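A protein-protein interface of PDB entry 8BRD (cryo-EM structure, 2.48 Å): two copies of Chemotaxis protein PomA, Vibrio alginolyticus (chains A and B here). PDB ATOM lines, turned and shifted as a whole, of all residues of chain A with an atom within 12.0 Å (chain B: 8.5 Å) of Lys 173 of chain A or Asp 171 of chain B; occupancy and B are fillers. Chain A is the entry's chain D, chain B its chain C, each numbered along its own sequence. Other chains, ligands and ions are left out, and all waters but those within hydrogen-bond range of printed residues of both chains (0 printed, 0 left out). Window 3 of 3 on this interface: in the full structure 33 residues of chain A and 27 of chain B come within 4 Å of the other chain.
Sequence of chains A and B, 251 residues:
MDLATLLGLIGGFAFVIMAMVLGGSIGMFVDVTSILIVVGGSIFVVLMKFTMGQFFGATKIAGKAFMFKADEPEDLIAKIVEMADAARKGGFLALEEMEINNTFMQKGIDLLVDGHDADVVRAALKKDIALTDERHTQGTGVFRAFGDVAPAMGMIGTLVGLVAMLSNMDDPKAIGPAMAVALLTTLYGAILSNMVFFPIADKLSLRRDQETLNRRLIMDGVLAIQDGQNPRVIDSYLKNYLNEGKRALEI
O of Leu 166 of chain B lies close to N of Pro 177 of chain A (3.3 Å). O of Gly 176 of chain A sits close to O of Leu 166 of chain B, at 3.3 Å. The side-chain amino group (NZ) of Lys 173 of chain A lies within salt-bridge range of the side-chain carboxylate (OD1) of Asp 171 of chain B, at 3.7 Å. The backbone carbonyl oxygen (O) of Lys 173 of chain A sits close to the side-chain carboxylate (OD1) of Asp 170 of chain B (3.2 Å).
N of Lys 173 of chain A lies within hydrogen-bond range of OD1 of Asp 171 of chain A, at 3.3 Å.
Among the printed residues, merely in contact across the chains: Lys 173 of chain A with Met 169 of chain B, Gly 176 of chain A with Met 169 of chain B, Pro 177 of chain A with Ser 167 of chain B, Met 179 of chain A with Leu 166 of chain B, Met 179 of chain A with Met 169 of chain B, Ala 180 of chain A with Leu 166 of chain B and Ala 180 of chain A with Ser 167 of chain B.
Lys 173 of chain A touches three residues of chain B. Ala 174 of chain A touches none of the printed residues of chain B. Ile 175 of chain A touches none of the printed residues of chain B. Of the printed residues of chain B, Met 179 of chain A touches Leu 166 and Met 169. Printed residues of chain B within 4 Å of Ala 180 of chain A: Leu 166 and Ser 167. Printed residues of chain A within 4 Å of Leu 166 of chain B: Gly 176, Pro 177, Met 179 and Ala 180. Of the printed residues of chain A, Ser 167 of chain B touches Pro 177 and Ala 180. No residue of chain A comes within 4 Å of Pro 172 of chain B. No residue of chain A comes within 4 Å of Lys 173 of chain B. No residue of chain A comes within 4 Å of Ala 174 of chain B. The nearest residue of chain B that does not touch Lys 173 of chain A is Leu 166 of chain B (6.5 Å). The nearest printed residue of chain B that does not touch Pro 177 of chain A is Met 169 of chain B (4.2 Å).
Of the 10 printed residues of chain B, 5 touch a printed residue of chain A. Hydrophobic or aromatic side chains of chain B within 4 Å of the printed part of chain A: Leu 166 and Met 169. Hydrophobic or aromatic side chains of chain A that line the printed part of chain B: Pro 177, Met 179 and Ala 180. Among the printed residues, 11 pairs touch across the chains. Among the printed residues, Asp or Glu carboxylates within 4 Å of a Lys or Arg side-chain nitrogen of the other chain: Lys 173 of chain A with Asp 171 of chain B.
Lys 173 of chain A touches Met 169 of chain B, but with the chains exchanged Met 169 of chain A does not touch Lys 173 of chain B (15.5 Å). Lys 173 of chain A touches Asp 170 of chain B, but with the chains exchanged Asp 170 of chain A does not touch Lys 173 of chain B (17.5 Å). Lys 173 of chain A touches Asp 171 of chain B, but with the chains exchanged Asp 171 of chain A does not touch Lys 173 of chain B (13.9 Å). Of the 11 pairs that touch across the chains among the printed residues, none has its exchanged pair printed and touching as well.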
ATOM      1  N   MET A 165      19.085  -4.218  20.859  1.00  0.00           N
ATOM      2  CA  MET A 165      17.939  -3.641  21.552  1.00  0.00           C
ATOM      3  C   MET A 165      17.411  -4.588  22.621  1.00  0.00           C
ATOM      4  O   MET A 165      17.040  -4.152  23.717  1.00  0.00           O
ATOM      5  CB  MET A 165      16.842  -3.293  20.548  1.00  0.00           C
ATOM      6  CG  MET A 165      15.472  -3.107  21.169  1.00  0.00           C
ATOM      7  SD  MET A 165      14.114  -3.300  20.010  1.00  0.00           S
ATOM      8  CE  MET A 165      13.625  -4.974  20.361  1.00  0.00           C
ATOM      9  N   LEU A 166      17.368  -5.887  22.322  1.00  0.00           N
ATOM     10  CA  LEU A 166      16.908  -6.866  23.298  1.00  0.00           C
ATOM     11  C   LEU A 166      17.918  -7.103  24.410  1.00  0.00           C
ATOM     12  O   LEU A 166      17.533  -7.556  25.491  1.00  0.00           O
ATOM     13  CB  LEU A 166      16.587  -8.184  22.601  1.00  0.00           C
ATOM     14  CG  LEU A 166      15.349  -8.141  21.716  1.00  0.00           C
ATOM     15  CD1 LEU A 166      15.147  -9.467  21.029  1.00  0.00           C
ATOM     16  CD2 LEU A 166      14.153  -7.793  22.563  1.00  0.00           C
ATOM     17  N   ASN A 168      19.464  -4.882  26.133  1.00  0.00           N
ATOM     18  CA  ASN A 168      19.187  -3.940  27.216  1.00  0.00           C
ATOM     19  C   ASN A 168      17.926  -3.166  26.843  1.00  0.00           C
ATOM     20  O   ASN A 168      18.000  -2.155  26.140  1.00  0.00           O
ATOM     21  CB  ASN A 168      20.372  -3.012  27.454  1.00  0.00           C
ATOM     22  CG  ASN A 168      20.938  -2.441  26.170  1.00  0.00           C
ATOM     23  OD1 ASN A 168      21.860  -3.004  25.581  1.00  0.00           O
ATOM     24  ND2 ASN A 168      20.388  -1.317  25.732  1.00  0.00           N
ATOM     25  N   MET A 169      16.777  -3.641  27.319  1.00  0.00           N
ATOM     26  CA  MET A 169      15.500  -3.009  26.976  1.00  0.00           C
ATOM     27  C   MET A 169      15.250  -1.798  27.870  1.00  0.00           C
ATOM     28  O   MET A 169      15.217  -0.660  27.393  1.00  0.00           O
ATOM     29  CB  MET A 169      14.371  -4.035  27.088  1.00  0.00           C
ATOM     30  CG  MET A 169      14.506  -5.201  26.124  1.00  0.00           C
ATOM     31  SD  MET A 169      12.925  -5.802  25.512  1.00  0.00           S
ATOM     32  CE  MET A 169      12.625  -7.174  26.614  1.00  0.00           C
ATOM     33  N   ASP A 170      15.051  -2.038  29.168  1.00  0.00           N
ATOM     34  CA  ASP A 170      15.053  -1.003  30.201  1.00  0.00           C
ATOM     35  C   ASP A 170      13.868  -0.051  30.032  1.00  0.00           C
ATOM     36  O   ASP A 170      13.501   0.662  30.970  1.00  0.00           O
ATOM     37  CB  ASP A 170      16.438  -0.311  30.175  1.00  0.00           C
ATOM     38  CG  ASP A 170      16.514   1.027  30.934  1.00  0.00           C
ATOM     39  OD1 ASP A 170      15.614   1.887  30.881  1.00  0.00           O
ATOM     40  OD2 ASP A 170      17.594   1.273  31.508  1.00  0.00           O
ATOM     41  N   ASP A 171      13.176  -0.125  28.901  1.00  0.00           N
ATOM     42  CA  ASP A 171      12.083   0.795  28.615  1.00  0.00           C
ATOM     43  C   ASP A 171      11.199   0.209  27.521  1.00  0.00           C
ATOM     44  O   ASP A 171      11.689  -0.107  26.429  1.00  0.00           O
ATOM     45  CB  ASP A 171      12.632   2.161  28.196  1.00  0.00           C
ATOM     46  CG  ASP A 171      11.577   3.251  28.215  1.00  0.00           C
ATOM     47  OD1 ASP A 171      10.395   2.942  28.466  1.00  0.00           O
ATOM     48  OD2 ASP A 171      11.935   4.425  27.985  1.00  0.00           O
ATOM     49  N   PRO A 172       9.898   0.045  27.773  1.00  0.00           N
ATOM     50  CA  PRO A 172       9.034  -0.524  26.727  1.00  0.00           C
ATOM     51  C   PRO A 172       8.654   0.473  25.649  1.00  0.00           C
ATOM     52  O   PRO A 172       8.471   0.081  24.490  1.00  0.00           O
ATOM     53  CB  PRO A 172       7.810  -1.006  27.515  1.00  0.00           C
ATOM     54  CG  PRO A 172       7.805  -0.186  28.752  1.00  0.00           C
ATOM     55  CD  PRO A 172       9.237   0.070  29.088  1.00  0.00           C
ATOM     56  N   LYS A 173       8.520   1.754  25.989  1.00  0.00           N
ATOM     57  CA  LYS A 173       8.164   2.755  24.993  1.00  0.00           C
ATOM     58  C   LYS A 173       9.289   3.038  24.011  1.00  0.00           C
ATOM     59  O   LYS A 173       9.054   3.705  23.001  1.00  0.00           O
ATOM     60  CB  LYS A 173       7.740   4.058  25.673  1.00  0.00           C
ATOM     61  CG  LYS A 173       6.371   3.993  26.323  1.00  0.00           C
ATOM     62  CD  LYS A 173       5.918   5.361  26.796  1.00  0.00           C
ATOM     63  CE  LYS A 173       4.513   5.302  27.369  1.00  0.00           C
ATOM     64  NZ  LYS A 173       3.687   6.457  26.920  1.00  0.00           N
ATOM     65  N   ALA A 174      10.496   2.558  24.286  1.00  0.00           N
ATOM     66  CA  ALA A 174      11.622   2.693  23.376  1.00  0.00           C
ATOM     67  C   ALA A 174      11.812   1.473  22.487  1.00  0.00           C
ATOM     68  O   ALA A 174      12.765   1.441  21.703  1.00  0.00           O
ATOM     69  CB  ALA A 174      12.905   2.964  24.167  1.00  0.00           C
ATOM     70  N   ILE A 175      10.941   0.469  22.597  1.00  0.00           N
ATOM     71  CA  ILE A 175      11.092  -0.740  21.792  1.00  0.00           C
ATOM     72  C   ILE A 175      10.858  -0.437  20.318  1.00  0.00           C
ATOM     73  O   ILE A 175      11.675  -0.791  19.461  1.00  0.00           O
ATOM     74  CB  ILE A 175      10.142  -1.842  22.296  1.00  0.00           C
ATOM     75  CG1 ILE A 175      10.512  -2.258  23.715  1.00  0.00           C
ATOM     76  CG2 ILE A 175      10.200  -3.047  21.380  1.00  0.00           C
ATOM     77  CD1 ILE A 175      11.842  -2.942  23.804  1.00  0.00           C
ATOM     78  N   GLY A 176       9.757   0.242  20.006  1.00  0.00           N
ATOM     79  CA  GLY A 176       9.378   0.519  18.640  1.00  0.00           C
ATOM     80  C   GLY A 176      10.391   1.318  17.844  1.00  0.00           C
ATOM     81  O   GLY A 176      10.788   0.921  16.745  1.00  0.00           O
ATOM     82  N   PRO A 177      10.819   2.472  18.369  1.00  0.00           N
ATOM     83  CA  PRO A 177      11.852   3.248  17.662  1.00  0.00           C
ATOM     84  C   PRO A 177      13.145   2.482  17.435  1.00  0.00           C
ATOM     85  O   PRO A 177      13.796   2.652  16.392  1.00  0.00           O
ATOM     86  CB  PRO A 177      12.049   4.457  18.580  1.00  0.00           C
ATOM     87  CG  PRO A 177      10.741   4.626  19.241  1.00  0.00           C
ATOM     88  CD  PRO A 177      10.221   3.245  19.472  1.00  0.00           C
ATOM     89  N   ALA A 178      13.536   1.633  18.385  1.00  0.00           N
ATOM     90  CA  ALA A 178      14.740   0.829  18.206  1.00  0.00           C
ATOM     91  C   ALA A 178      14.591  -0.128  17.031  1.00  0.00           C
ATOM     92  O   ALA A 178      15.514  -0.278  16.221  1.00  0.00           O
ATOM     93  CB  ALA A 178      15.059   0.073  19.493  1.00  0.00           C
ATOM     94  N   MET A 179      13.431  -0.781  16.906  1.00  0.00           N
ATOM     95  CA  MET A 179      13.217  -1.664  15.764  1.00  0.00           C
ATOM     96  C   MET A 179      13.110  -0.882  14.464  1.00  0.00           C
ATOM     97  O   MET A 179      13.502  -1.376  13.406  1.00  0.00           O
ATOM     98  CB  MET A 179      11.984  -2.551  15.954  1.00  0.00           C
ATOM     99  CG  MET A 179      11.700  -2.990  17.366  1.00  0.00           C
ATOM    100  SD  MET A 179      10.600  -4.421  17.380  1.00  0.00           S
ATOM    101  CE  MET A 179       9.108  -3.727  18.065  1.00  0.00           C
ATOM    102  N   ALA A 180      12.580   0.339  14.518  1.00  0.00           N
ATOM    103  CA  ALA A 180      12.555   1.176  13.320  1.00  0.00           C
ATOM    104  C   ALA A 180      13.967   1.471  12.830  1.00  0.00           C
ATOM    105  O   ALA A 180      14.278   1.323  11.638  1.00  0.00           O
ATOM    106  CB  ALA A 180      11.801   2.473  13.609  1.00  0.00           C
ATOM    107  N   VAL A 181      14.848   1.868  13.751  1.00  0.00           N
ATOM    108  CA  VAL A 181      16.237   2.131  13.384  1.00  0.00           C
ATOM    109  C   VAL A 181      16.909   0.858  12.881  1.00  0.00           C
ATOM    110  O   VAL A 181      17.673   0.886  11.910  1.00  0.00           O
ATOM    111  CB  VAL A 181      17.004   2.746  14.568  1.00  0.00           C
ATOM    112  CG1 VAL A 181      18.447   2.991  14.185  1.00  0.00           C
ATOM    113  CG2 VAL A 181      16.349   4.037  15.004  1.00  0.00           C
ATOM    114  N   LEU B 166       6.612   1.824  13.582  1.00  0.00           N
ATOM    115  CA  LEU B 166       7.407   1.502  14.759  1.00  0.00           C
ATOM    116  C   LEU B 166       7.954   2.759  15.423  1.00  0.00           C
ATOM    117  O   LEU B 166       8.066   2.813  16.650  1.00  0.00           O
ATOM    118  CB  LEU B 166       8.538   0.550  14.383  1.00  0.00           C
ATOM    119  CG  LEU B 166       8.112  -0.844  13.915  1.00  0.00           C
ATOM    120  CD1 LEU B 166       9.280  -1.573  13.293  1.00  0.00           C
ATOM    121  CD2 LEU B 166       7.527  -1.646  15.059  1.00  0.00           C
ATOM    122  N   SER B 167       8.302   3.778  14.634  1.00  0.00           N
ATOM    123  CA  SER B 167       8.801   5.015  15.226  1.00  0.00           C
ATOM    124  C   SER B 167       7.748   5.687  16.099  1.00  0.00           C
ATOM    125  O   SER B 167       8.091   6.362  17.075  1.00  0.00           O
ATOM    126  CB  SER B 167       9.263   5.977  14.136  1.00  0.00           C
ATOM    127  OG  SER B 167       9.821   5.277  13.043  1.00  0.00           O
ATOM    128  N   ASN B 168       6.472   5.515  15.768  1.00  0.00           N
ATOM    129  CA  ASN B 168       5.374   6.100  16.526  1.00  0.00           C
ATOM    130  C   ASN B 168       4.654   5.056  17.371  1.00  0.00           C
ATOM    131  O   ASN B 168       3.447   5.156  17.597  1.00  0.00           O
ATOM    132  CB  ASN B 168       4.390   6.795  15.587  1.00  0.00           C
ATOM    133  CG  ASN B 168       5.056   7.839  14.720  1.00  0.00           C
ATOM    134  OD1 ASN B 168       5.095   7.714  13.495  1.00  0.00           O
ATOM    135  ND2 ASN B 168       5.591   8.877  15.349  1.00  0.00           N
ATOM    136  N   MET B 169       5.383   4.049  17.840  1.00  0.00           N
ATOM    137  CA  MET B 169       4.800   2.931  18.574  1.00  0.00           C
ATOM    138  C   MET B 169       5.082   3.111  20.061  1.00  0.00           C
ATOM    139  O   MET B 169       6.188   2.833  20.534  1.00  0.00           O
ATOM    140  CB  MET B 169       5.349   1.602  18.072  1.00  0.00           C
ATOM    141  CG  MET B 169       4.602   0.406  18.622  1.00  0.00           C
ATOM    142  SD  MET B 169       5.093  -1.147  17.866  1.00  0.00           S
ATOM    143  CE  MET B 169       6.434  -1.608  18.948  1.00  0.00           C
ATOM    144  N   ASP B 170       4.077   3.578  20.794  1.00  0.00           N
ATOM    145  CA  ASP B 170       4.071   3.562  22.250  1.00  0.00           C
ATOM    146  C   ASP B 170       2.860   2.755  22.690  1.00  0.00           C
ATOM    147  O   ASP B 170       1.730   3.077  22.304  1.00  0.00           O
ATOM    148  CB  ASP B 170       4.013   4.979  22.825  1.00  0.00           C
ATOM    149  CG  ASP B 170       5.335   5.706  22.717  1.00  0.00           C
ATOM    150  OD1 ASP B 170       6.307   5.102  22.214  1.00  0.00           O
ATOM    151  OD2 ASP B 170       5.406   6.882  23.131  1.00  0.00           O
ATOM    152  N   ASP B 171       3.096   1.706  23.486  1.00  0.00           N
ATOM    153  CA  ASP B 171       2.017   0.831  23.938  1.00  0.00           C
ATOM    154  C   ASP B 171       1.294   0.257  22.726  1.00  0.00           C
ATOM    155  O   ASP B 171       0.183   0.693  22.402  1.00  0.00           O
ATOM    156  CB  ASP B 171       1.048   1.575  24.857  1.00  0.00           C
ATOM    157  CG  ASP B 171       1.723   2.108  26.107  1.00  0.00           C
ATOM    158  OD1 ASP B 171       2.383   3.164  26.024  1.00  0.00           O
ATOM    159  OD2 ASP B 171       1.600   1.464  27.170  1.00  0.00           O
ATOM    160  N   PRO B 172       1.895  -0.713  22.028  1.00  0.00           N
ATOM    161  CA  PRO B 172       1.428  -1.060  20.679  1.00  0.00           C
ATOM    162  C   PRO B 172       0.049  -1.647  20.931  1.00  0.00           C
ATOM    163  O   PRO B 172      -0.085  -2.827  21.268  1.00  0.00           O
ATOM    164  CB  PRO B 172       2.493  -2.049  20.194  1.00  0.00           C
ATOM    165  CG  PRO B 172       2.990  -2.689  21.443  1.00  0.00           C
ATOM    166  CD  PRO B 172       2.952  -1.622  22.501  1.00  0.00           C
ATOM    167  N   LYS B 173      -0.987  -0.828  20.755  1.00  0.00           N
ATOM    168  CA  LYS B 173      -2.354  -1.330  20.750  1.00  0.00           C
ATOM    169  C   LYS B 173      -3.091  -0.367  19.828  1.00  0.00           C
ATOM    170  O   LYS B 173      -4.325  -0.413  19.766  1.00  0.00           O
ATOM    171  CB  LYS B 173      -3.097  -1.473  22.081  1.00  0.00           C
ATOM    172  CG  LYS B 173      -3.233  -0.188  22.868  1.00  0.00           C
ATOM    173  CD  LYS B 173      -3.878  -0.443  24.222  1.00  0.00           C
ATOM    174  CE  LYS B 173      -5.070  -1.380  24.106  1.00  0.00           C
ATOM    175  NZ  LYS B 173      -5.316  -2.129  25.368  1.00  0.00           N
ATOM    176  N   ALA B 174      -2.370   0.503  19.119  1.00  0.00           N
ATOM    177  CA  ALA B 174      -2.948   1.376  18.107  1.00  0.00           C
ATOM    178  C   ALA B 174      -2.220   1.262  16.774  1.00  0.00           C
ATOM    179  O   ALA B 174      -2.450   2.086  15.883  1.00  0.00           O
ATOM    180  CB  ALA B 174      -2.945   2.833  18.578  1.00  0.00           C
ATOM    181  N   ILE B 175      -1.348   0.260  16.615  1.00  0.00           N
ATOM    182  CA  ILE B 175      -0.548   0.121  15.399  1.00  0.00           C
ATOM    183  C   ILE B 175      -1.283  -0.580  14.272  1.00  0.00           C
ATOM    184  O   ILE B 175      -0.698  -0.773  13.199  1.00  0.00           O
ATOM    185  CB  ILE B 175       0.755  -0.651  15.688  1.00  0.00           C
ATOM    186  CG1 ILE B 175       0.444  -2.109  16.026  1.00  0.00           C
ATOM    187  CG2 ILE B 175       1.518   0.008  16.816  1.00  0.00           C
ATOM    188  CD1 ILE B 175       1.659  -2.993  16.074  1.00  0.00           C
